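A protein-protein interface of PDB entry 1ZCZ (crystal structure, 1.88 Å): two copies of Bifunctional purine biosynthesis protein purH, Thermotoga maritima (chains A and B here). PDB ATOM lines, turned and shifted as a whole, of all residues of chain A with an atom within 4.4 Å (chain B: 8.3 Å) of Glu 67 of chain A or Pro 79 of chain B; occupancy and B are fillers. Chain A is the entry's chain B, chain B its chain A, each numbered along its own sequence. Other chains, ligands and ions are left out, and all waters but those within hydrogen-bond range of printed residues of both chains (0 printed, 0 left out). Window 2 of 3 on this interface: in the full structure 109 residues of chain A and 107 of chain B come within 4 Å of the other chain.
Glu 67 of chain A touches one residue of chain B. Printed residues of chain B within 4 Å of Leu 69 of chain A: Ala 83 (3.8 Å). Of the printed residues of chain B, Leu 77 of chain A touches Leu 77, His 78, Pro 79 and Phe 82. Thr 64 of chain B touches none of the printed residues of chain A. Gly 84 of chain B touches none of the printed residues of chain A. The nearest residue of chain B that does not touch Glu 67 of chain A is Glu 80 of chain B (6.2 Å).
Among the printed residues, merely in contact across the chains: Glu 67 of chain A with Pro 79 of chain B (3.8 Å), Leu 69 of chain A with Ala 83 of chain B (3.8 Å), Val 74 of chain A with Pro 79 of chain B (3.6 Å), Val 74 of chain A with Leu 86 of chain B (3.98 Å), Leu 77 of chain A with Leu 77 of chain B (3.5 Å), Leu 77 of chain A with His 78 of chain B (3.3 Å), Leu 77 of chain A with Phe 82 of chain B (3.8 Å), His 78 of chain A with Leu 77 of chain B (3.2 Å) and His 78 of chain A with Pro 79 of chain B (3.8 Å).
Of the 18 printed residues of chain B, 6 touch a printed residue of chain A. Printed residues of chain B that touch a printed residue of chain A: Leu 77, His 78, Pro 79, Phe 82, Ala 83 and Leu 86. Hydrophobic or aromatic side chains of chain A that line the printed part of chain B: Leu 69, Val 74, Leu 77 and His 78.
Leu 77 of chain A touches its own counterpart, Leu 77 of chain B. Leu 77 of chain A touches His 78 of chain B, and with the chains exchanged His 78 of chain A touches Leu 77 of chain B. Of the 10 pairs that touch across the chains among the printed residues, 3 have their exchanged pair printed and touching as well.
O of Leu 77 of chain A sits close to N of Pro 79 of chain B (3.1 Å).
OG1 of Thr 64 of chain B sits at hydrogen-bond distance from ND1 of His 78 of chain B (2.6 Å). O of Val 74 of chain B lies close to NE2 of His 78 of chain B (3.4 Å). NE2 of His 78 of chain B sits close to O of Lys 75 of chain B, 3.3 Å away. The side-chain carboxylate of Glu 67 of chain A sits at hydrogen-bond distance from the backbone NH of Leu 69 of chain A (2.9 Å). The side-chain carboxylate (OE2) of Glu 67 of chain A sits close to the backbone NH (N) of Lys 75 of chain A, at 3.4 Å. The side-chain carboxylate (OE2) of Glu 67 of chain A is in hydrogen-bond range of a ring nitrogen (NE2) of His 78 of chain A.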
ATOM      1  N   GLY A  65      -6.585 -15.918 -18.069  1.00  0.00           N
ATOM      2  CA  GLY A  65      -7.104 -15.744 -16.726  1.00  0.00           C
ATOM      3  C   GLY A  65      -6.074 -16.108 -15.683  1.00  0.00           C
ATOM      4  O   GLY A  65      -5.173 -16.895 -15.951  1.00  0.00           O
ATOM      5  N   PHE A  66      -6.207 -15.530 -14.493  1.00  0.00           N
ATOM      6  CA  PHE A  66      -5.286 -15.804 -13.406  1.00  0.00           C
ATOM      7  C   PHE A  66      -5.830 -16.901 -12.490  1.00  0.00           C
ATOM      8  O   PHE A  66      -7.013 -16.885 -12.072  1.00  0.00           O
ATOM      9  CB  PHE A  66      -5.018 -14.541 -12.565  1.00  0.00           C
ATOM     10  CG  PHE A  66      -3.967 -14.765 -11.510  1.00  0.00           C
ATOM     11  CD1 PHE A  66      -4.364 -14.979 -10.169  1.00  0.00           C
ATOM     12  CD2 PHE A  66      -2.561 -14.822 -11.874  1.00  0.00           C
ATOM     13  CE1 PHE A  66      -3.389 -15.204  -9.201  1.00  0.00           C
ATOM     14  CE2 PHE A  66      -1.578 -15.056 -10.910  1.00  0.00           C
ATOM     15  CZ  PHE A  66      -1.997 -15.241  -9.567  1.00  0.00           C
ATOM     16  N   GLU A  67      -4.952 -17.827 -12.143  1.00  0.00           N
ATOM     17  CA  GLU A  67      -5.280 -18.830 -11.142  1.00  0.00           C
ATOM     18  C   GLU A  67      -4.043 -19.166 -10.320  1.00  0.00           C
ATOM     19  O   GLU A  67      -2.911 -19.079 -10.803  1.00  0.00           O
ATOM     20  CB  GLU A  67      -5.919 -20.082 -11.767  1.00  0.00           C
ATOM     21  CG  GLU A  67      -5.172 -20.676 -12.950  1.00  0.00           C
ATOM     22  CD  GLU A  67      -3.882 -21.389 -12.561  1.00  0.00           C
ATOM     23  OE1 GLU A  67      -3.754 -21.913 -11.403  1.00  0.00           O
ATOM     24  OE2 GLU A  67      -2.977 -21.427 -13.411  1.00  0.00           O
ATOM     25  N   ASN A  68      -4.279 -19.505  -9.058  1.00  0.00           N
ATOM     26  CA  ASN A  68      -3.230 -19.654  -8.079  1.00  0.00           C
ATOM     27  C   ASN A  68      -3.209 -21.114  -7.614  1.00  0.00           C
ATOM     28  O   ASN A  68      -2.765 -21.446  -6.508  1.00  0.00           O
ATOM     29  CB  ASN A  68      -3.531 -18.686  -6.935  1.00  0.00           C
ATOM     30  CG  ASN A  68      -2.415 -18.567  -5.930  1.00  0.00           C
ATOM     31  OD1 ASN A  68      -2.670 -18.343  -4.741  1.00  0.00           O
ATOM     32  ND2 ASN A  68      -1.169 -18.676  -6.378  1.00  0.00           N
ATOM     33  N   LEU A  69      -3.710 -21.991  -8.477  1.00  0.00           N
ATOM     34  CA  LEU A  69      -3.788 -23.397  -8.123  1.00  0.00           C
ATOM     35  C   LEU A  69      -2.377 -23.994  -7.993  1.00  0.00           C
ATOM     36  O   LEU A  69      -1.519 -23.786  -8.858  1.00  0.00           O
ATOM     37  CB  LEU A  69      -4.636 -24.160  -9.143  1.00  0.00           C
ATOM     38  CG  LEU A  69      -6.073 -23.637  -9.265  1.00  0.00           C
ATOM     39  CD1 LEU A  69      -6.775 -24.297 -10.426  1.00  0.00           C
ATOM     40  CD2 LEU A  69      -6.853 -23.845  -7.964  1.00  0.00           C
ATOM     41  N   VAL A  74       0.161 -25.069 -12.679  1.00  0.00           N
ATOM     42  CA  VAL A  74      -0.609 -25.197 -13.936  1.00  0.00           C
ATOM     43  C   VAL A  74      -0.859 -23.909 -14.714  1.00  0.00           C
ATOM     44  O   VAL A  74      -1.734 -23.869 -15.562  1.00  0.00           O
ATOM     45  CB  VAL A  74      -1.935 -25.955 -13.714  1.00  0.00           C
ATOM     46  CG1 VAL A  74      -1.645 -27.290 -13.097  1.00  0.00           C
ATOM     47  CG2 VAL A  74      -2.909 -25.147 -12.847  1.00  0.00           C
ATOM     48  N   LYS A  75      -0.072 -22.873 -14.447  1.00  0.00           N
ATOM     49  CA  LYS A  75      -0.264 -21.579 -15.107  1.00  0.00           C
ATOM     50  C   LYS A  75       0.027 -21.532 -16.614  1.00  0.00           C
ATOM     51  O   LYS A  75      -0.409 -20.609 -17.292  1.00  0.00           O
ATOM     52  CB  LYS A  75       0.452 -20.450 -14.338  1.00  0.00           C
ATOM     53  CG  LYS A  75       1.950 -20.585 -14.151  1.00  0.00           C
ATOM     54  CD  LYS A  75       2.740 -19.932 -15.260  1.00  0.00           C
ATOM     55  CE  LYS A  75       4.168 -19.609 -14.817  1.00  0.00           C
ATOM     56  NZ  LYS A  75       5.031 -20.821 -14.727  1.00  0.00           N
ATOM     57  N   LEU A  77      -0.977 -24.148 -18.479  1.00  0.00           N
ATOM     58  CA  LEU A  77      -2.028 -25.026 -18.993  1.00  0.00           C
ATOM     59  C   LEU A  77      -3.374 -24.280 -19.040  1.00  0.00           C
ATOM     60  O   LEU A  77      -4.332 -24.631 -18.354  1.00  0.00           O
ATOM     61  CB  LEU A  77      -2.093 -26.299 -18.150  1.00  0.00           C
ATOM     62  CG  LEU A  77      -0.872 -27.228 -18.341  1.00  0.00           C
ATOM     63  CD1 LEU A  77      -0.637 -28.098 -17.125  1.00  0.00           C
ATOM     64  CD2 LEU A  77      -1.007 -28.086 -19.624  1.00  0.00           C
ATOM     65  N   HIS A  78      -3.409 -23.238 -19.868  1.00  0.00           N
ATOM     66  CA  HIS A  78      -4.552 -22.365 -20.012  1.00  0.00           C
ATOM     67  C   HIS A  78      -5.000 -22.355 -21.490  1.00  0.00           C
ATOM     68  O   HIS A  78      -4.157 -22.459 -22.381  1.00  0.00           O
ATOM     69  CB  HIS A  78      -4.130 -20.951 -19.578  1.00  0.00           C
ATOM     70  CG  HIS A  78      -3.997 -20.771 -18.091  1.00  0.00           C
ATOM     71  ND1 HIS A  78      -4.305 -19.583 -17.459  1.00  0.00           N
ATOM     72  CD2 HIS A  78      -3.610 -21.624 -17.114  1.00  0.00           C
ATOM     73  CE1 HIS A  78      -4.097 -19.707 -16.165  1.00  0.00           C
ATOM     74  NE2 HIS A  78      -3.675 -20.933 -15.927  1.00  0.00           N
ATOM     75  N   ILE B  63     -16.784 -27.807 -14.224  1.00  0.00           N
ATOM     76  CA  ILE B  63     -15.774 -27.310 -13.280  1.00  0.00           C
ATOM     77  C   ILE B  63     -14.758 -26.340 -13.907  1.00  0.00           C
ATOM     78  O   ILE B  63     -13.720 -26.058 -13.292  1.00  0.00           O
ATOM     79  CB  ILE B  63     -14.968 -28.490 -12.637  1.00  0.00           C
ATOM     80  CG1 ILE B  63     -14.129 -29.228 -13.664  1.00  0.00           C
ATOM     81  CG2 ILE B  63     -15.894 -29.482 -11.992  1.00  0.00           C
ATOM     82  CD1 ILE B  63     -13.108 -30.195 -13.035  1.00  0.00           C
ATOM     83  N   THR B  64     -15.022 -25.871 -15.135  1.00  0.00           N
ATOM     84  CA  THR B  64     -14.149 -24.898 -15.800  1.00  0.00           C
ATOM     85  C   THR B  64     -14.938 -23.778 -16.488  1.00  0.00           C
ATOM     86  O   THR B  64     -16.139 -23.916 -16.741  1.00  0.00           O
ATOM     87  CB  THR B  64     -13.236 -25.589 -16.823  1.00  0.00           C
ATOM     88  OG1 THR B  64     -12.170 -24.698 -17.185  1.00  0.00           O
ATOM     89  CG2 THR B  64     -14.026 -26.037 -18.083  1.00  0.00           C
ATOM     90  N   GLY B  65     -14.268 -22.664 -16.780  1.00  0.00           N
ATOM     91  CA  GLY B  65     -14.911 -21.561 -17.522  1.00  0.00           C
ATOM     92  C   GLY B  65     -15.177 -21.975 -18.965  1.00  0.00           C
ATOM     93  O   GLY B  65     -14.278 -22.513 -19.632  1.00  0.00           O
ATOM     94  N   VAL B  74      -9.367 -26.736 -27.728  1.00  0.00           N
ATOM     95  CA  VAL B  74      -8.623 -26.523 -26.471  1.00  0.00           C
ATOM     96  C   VAL B  74      -9.465 -26.674 -25.188  1.00  0.00           C
ATOM     97  O   VAL B  74      -9.045 -26.275 -24.114  1.00  0.00           O
ATOM     98  CB  VAL B  74      -7.885 -25.146 -26.535  1.00  0.00           C
ATOM     99  CG1 VAL B  74      -8.850 -24.015 -26.551  1.00  0.00           C
ATOM    100  CG2 VAL B  74      -6.859 -25.007 -25.404  1.00  0.00           C
ATOM    101  N   LYS B  75     -10.660 -27.258 -25.328  1.00  0.00           N
ATOM    102  CA  LYS B  75     -11.579 -27.528 -24.221  1.00  0.00           C
ATOM    103  C   LYS B  75     -10.931 -28.283 -23.039  1.00  0.00           C
ATOM    104  O   LYS B  75     -11.336 -28.095 -21.886  1.00  0.00           O
ATOM    105  CB  LYS B  75     -12.793 -28.323 -24.740  1.00  0.00           C
ATOM    106  CG  LYS B  75     -13.756 -27.514 -25.641  1.00  0.00           C
ATOM    107  N   THR B  76      -9.930 -29.117 -23.315  1.00  0.00           N
ATOM    108  CA  THR B  76      -9.274 -29.925 -22.273  1.00  0.00           C
ATOM    109  C   THR B  76      -8.096 -29.203 -21.558  1.00  0.00           C
ATOM    110  O   THR B  76      -7.738 -29.542 -20.400  1.00  0.00           O
ATOM    111  CB  THR B  76      -8.770 -31.281 -22.896  1.00  0.00           C
ATOM    112  OG1 THR B  76      -9.909 -32.116 -23.175  1.00  0.00           O
ATOM    113  CG2 THR B  76      -7.822 -31.987 -21.971  1.00  0.00           C
ATOM    114  N   LEU B  77      -7.522 -28.207 -22.233  1.00  0.00           N
ATOM    115  CA  LEU B  77      -6.287 -27.540 -21.764  1.00  0.00           C
ATOM    116  C   LEU B  77      -6.632 -26.374 -20.816  1.00  0.00           C
ATOM    117  O   LEU B  77      -6.433 -25.202 -21.125  1.00  0.00           O
ATOM    118  CB  LEU B  77      -5.462 -27.086 -22.956  1.00  0.00           C
ATOM    119  CG  LEU B  77      -4.788 -28.275 -23.665  1.00  0.00           C
ATOM    120  CD1 LEU B  77      -4.648 -27.999 -25.184  1.00  0.00           C
ATOM    121  CD2 LEU B  77      -3.434 -28.579 -23.037  1.00  0.00           C
ATOM    122  N   HIS B  78      -7.170 -26.757 -19.661  1.00  0.00           N
ATOM    123  CA  HIS B  78      -7.706 -25.832 -18.677  1.00  0.00           C
ATOM    124  C   HIS B  78      -7.077 -26.162 -17.313  1.00  0.00           C
ATOM    125  O   HIS B  78      -6.885 -27.356 -16.982  1.00  0.00           O
ATOM    126  CB  HIS B  78      -9.227 -26.000 -18.566  1.00  0.00           C
ATOM    127  CG  HIS B  78     -10.010 -25.412 -19.704  1.00  0.00           C
ATOM    128  ND1 HIS B  78     -11.023 -24.505 -19.506  1.00  0.00           N
ATOM    129  CD2 HIS B  78      -9.971 -25.646 -21.038  1.00  0.00           C
ATOM    130  CE1 HIS B  78     -11.553 -24.175 -20.673  1.00  0.00           C
ATOM    131  NE2 HIS B  78     -10.928 -24.853 -21.618  1.00  0.00           N
ATOM    132  N   PRO B  79      -6.764 -25.118 -16.507  1.00  0.00           N
ATOM    133  CA  PRO B  79      -5.996 -25.331 -15.264  1.00  0.00           C
ATOM    134  C   PRO B  79      -6.758 -26.150 -14.207  1.00  0.00           C
ATOM    135  O   PRO B  79      -6.157 -26.932 -13.486  1.00  0.00           O
ATOM    136  CB  PRO B  79      -5.689 -23.906 -14.797  1.00  0.00           C
ATOM    137  CG  PRO B  79      -6.841 -23.053 -15.393  1.00  0.00           C
ATOM    138  CD  PRO B  79      -7.097 -23.699 -16.728  1.00  0.00           C
ATOM    139  N   GLU B  80      -8.075 -26.011 -14.151  1.00  0.00           N
ATOM    140  CA  GLU B  80      -8.866 -26.734 -13.145  1.00  0.00           C
ATOM    141  C   GLU B  80      -8.767 -28.238 -13.350  1.00  0.00           C
ATOM    142  O   GLU B  80      -8.718 -29.006 -12.369  1.00  0.00           O
ATOM    143  CB  GLU B  80     -10.332 -26.311 -13.170  1.00  0.00           C
ATOM    144  CG  GLU B  80     -10.542 -24.853 -12.883  1.00  0.00           C
ATOM    145  CD  GLU B  80     -10.585 -23.990 -14.133  1.00  0.00           C
ATOM    146  OE1 GLU B  80     -10.021 -24.390 -15.199  1.00  0.00           O
ATOM    147  OE2 GLU B  80     -11.194 -22.901 -14.024  1.00  0.00           O
ATOM    148  N   ILE B  81      -8.705 -28.660 -14.620  1.00  0.00           N
ATOM    149  CA  ILE B  81      -8.630 -30.072 -14.950  1.00  0.00           C
ATOM    150  C   ILE B  81      -7.242 -30.595 -14.555  1.00  0.00           C
ATOM    151  O   ILE B  81      -7.132 -31.583 -13.847  1.00  0.00           O
ATOM    152  CB  ILE B  81      -8.884 -30.359 -16.464  1.00  0.00           C
ATOM    153  CG1 ILE B  81     -10.238 -29.837 -16.945  1.00  0.00           C
ATOM    154  CG2 ILE B  81      -8.741 -31.864 -16.746  1.00  0.00           C
ATOM    155  CD1 ILE B  81     -11.423 -30.180 -16.069  1.00  0.00           C
ATOM    156  N   PHE B  82      -6.183 -29.911 -14.967  1.00  0.00           N
ATOM    157  CA  PHE B  82      -4.839 -30.374 -14.619  1.00  0.00           C
ATOM    158  C   PHE B  82      -4.538 -30.276 -13.122  1.00  0.00           C
ATOM    159  O   PHE B  82      -3.859 -31.143 -12.588  1.00  0.00           O
ATOM    160  CB  PHE B  82      -3.776 -29.691 -15.486  1.00  0.00           C
ATOM    161  CG  PHE B  82      -3.751 -30.239 -16.890  1.00  0.00           C
ATOM    162  CD1 PHE B  82      -4.614 -29.737 -17.865  1.00  0.00           C
ATOM    163  CD2 PHE B  82      -2.937 -31.310 -17.210  1.00  0.00           C
ATOM    164  CE1 PHE B  82      -4.628 -30.275 -19.141  1.00  0.00           C
ATOM    165  CE2 PHE B  82      -2.959 -31.850 -18.465  1.00  0.00           C
ATOM    166  CZ  PHE B  82      -3.798 -31.334 -19.437  1.00  0.00           C
ATOM    167  N   ALA B  83      -5.083 -29.277 -12.433  1.00  0.00           N
ATOM    168  CA  ALA B  83      -4.897 -29.195 -10.983  1.00  0.00           C
ATOM    169  C   ALA B  83      -5.597 -30.366 -10.282  1.00  0.00           C
ATOM    170  O   ALA B  83      -5.083 -30.906  -9.281  1.00  0.00           O
ATOM    171  CB  ALA B  83      -5.352 -27.871 -10.431  1.00  0.00           C
ATOM    172  N   GLY B  84      -6.740 -30.775 -10.824  1.00  0.00           N
ATOM    173  CA  GLY B  84      -7.496 -31.926 -10.293  1.00  0.00           C
ATOM    174  C   GLY B  84      -6.781 -33.266 -10.443  1.00  0.00           C
ATOM    175  O   GLY B  84      -7.161 -34.232  -9.785  1.00  0.00           O
ATOM    176  N   ILE B  85      -5.772 -33.330 -11.324  1.00  0.00           N
ATOM    177  CA  ILE B  85      -4.995 -34.545 -11.573  1.00  0.00           C
ATOM    178  C   ILE B  85      -3.670 -34.488 -10.826  1.00  0.00           C
ATOM    179  O   ILE B  85      -3.225 -35.504 -10.236  1.00  0.00           O
ATOM    180  CB  ILE B  85      -4.685 -34.719 -13.084  1.00  0.00           C
ATOM    181  CG1 ILE B  85      -5.966 -34.904 -13.890  1.00  0.00           C
ATOM    182  CG2 ILE B  85      -3.685 -35.879 -13.335  1.00  0.00           C
ATOM    183  CD1 ILE B  85      -5.785 -34.890 -15.414  1.00  0.00           C
ATOM    184  N   LEU B  86      -3.051 -33.303 -10.829  1.00  0.00           N
ATOM    185  CA  LEU B  86      -1.652 -33.140 -10.389  1.00  0.00           C
ATOM    186  C   LEU B  86      -1.479 -32.839  -8.908  1.00  0.00           C
ATOM    187  O   LEU B  86      -0.395 -32.997  -8.382  1.00  0.00           O
ATOM    188  CB  LEU B  86      -0.979 -32.027 -11.189  1.00  0.00           C
ATOM    189  CG  LEU B  86      -0.625 -32.308 -12.638  1.00  0.00           C
ATOM    190  CD1 LEU B  86      -0.235 -31.006 -13.297  1.00  0.00           C
ATOM    191  CD2 LEU B  86       0.545 -33.318 -12.735  1.00  0.00           C
ATOM    192  N   ARG B  91      -9.085 -34.937  -7.917  1.00  0.00           N
ATOM    193  CA  ARG B  91     -10.514 -35.122  -8.156  1.00  0.00           C
ATOM    194  C   ARG B  91     -10.851 -36.507  -8.667  1.00  0.00           C
ATOM    195  O   ARG B  91     -12.002 -36.920  -8.583  1.00  0.00           O
ATOM    196  CB  ARG B  91     -11.011 -34.138  -9.212  1.00  0.00           C
ATOM    197  CG  ARG B  91     -11.032 -32.703  -8.781  1.00  0.00           C
ATOM    198  CD  ARG B  91     -11.674 -31.883  -9.856  1.00  0.00           C
ATOM    199  NE  ARG B  91     -11.965 -30.535  -9.405  1.00  0.00           N
ATOM    200  CZ  ARG B  91     -13.178 -30.086  -9.095  1.00  0.00           C
ATOM    201  NH1 ARG B  91     -14.239 -30.882  -9.158  1.00  0.00           N
ATOM    202  NH2 ARG B  91     -13.317 -28.831  -8.696  1.00  0.00           N
ATOM    203  N   TRP B  92      -9.845 -37.209  -9.188  1.00  0.00           N
ATOM    204  CA  TRP B  92     -10.015 -38.467  -9.892  1.00  0.00           C
ATOM    205  C   TRP B  92      -8.969 -39.450  -9.431  1.00  0.00           C
ATOM    206  O   TRP B  92      -7.796 -39.096  -9.272  1.00  0.00           O
ATOM    207  CB  TRP B  92      -9.936 -38.250 -11.431  1.00  0.00           C
ATOM    208  CG  TRP B  92     -10.958 -37.244 -11.872  1.00  0.00           C
ATOM    209  CD1 TRP B  92     -12.311 -37.397 -11.872  1.00  0.00           C
ATOM    210  CD2 TRP B  92     -10.703 -35.907 -12.280  1.00  0.00           C
ATOM    211  NE1 TRP B  92     -12.915 -36.232 -12.275  1.00  0.00           N
ATOM    212  CE2 TRP B  92     -11.948 -35.307 -12.553  1.00  0.00           C
ATOM    213  CE3 TRP B  92      -9.538 -35.163 -12.480  1.00  0.00           C
ATOM    214  CZ2 TRP B  92     -12.059 -33.995 -13.010  1.00  0.00           C
ATOM    215  CZ3 TRP B  92      -9.650 -33.854 -12.934  1.00  0.00           C
ATOM    216  CH2 TRP B  92     -10.906 -33.278 -13.161  1.00  0.00           C
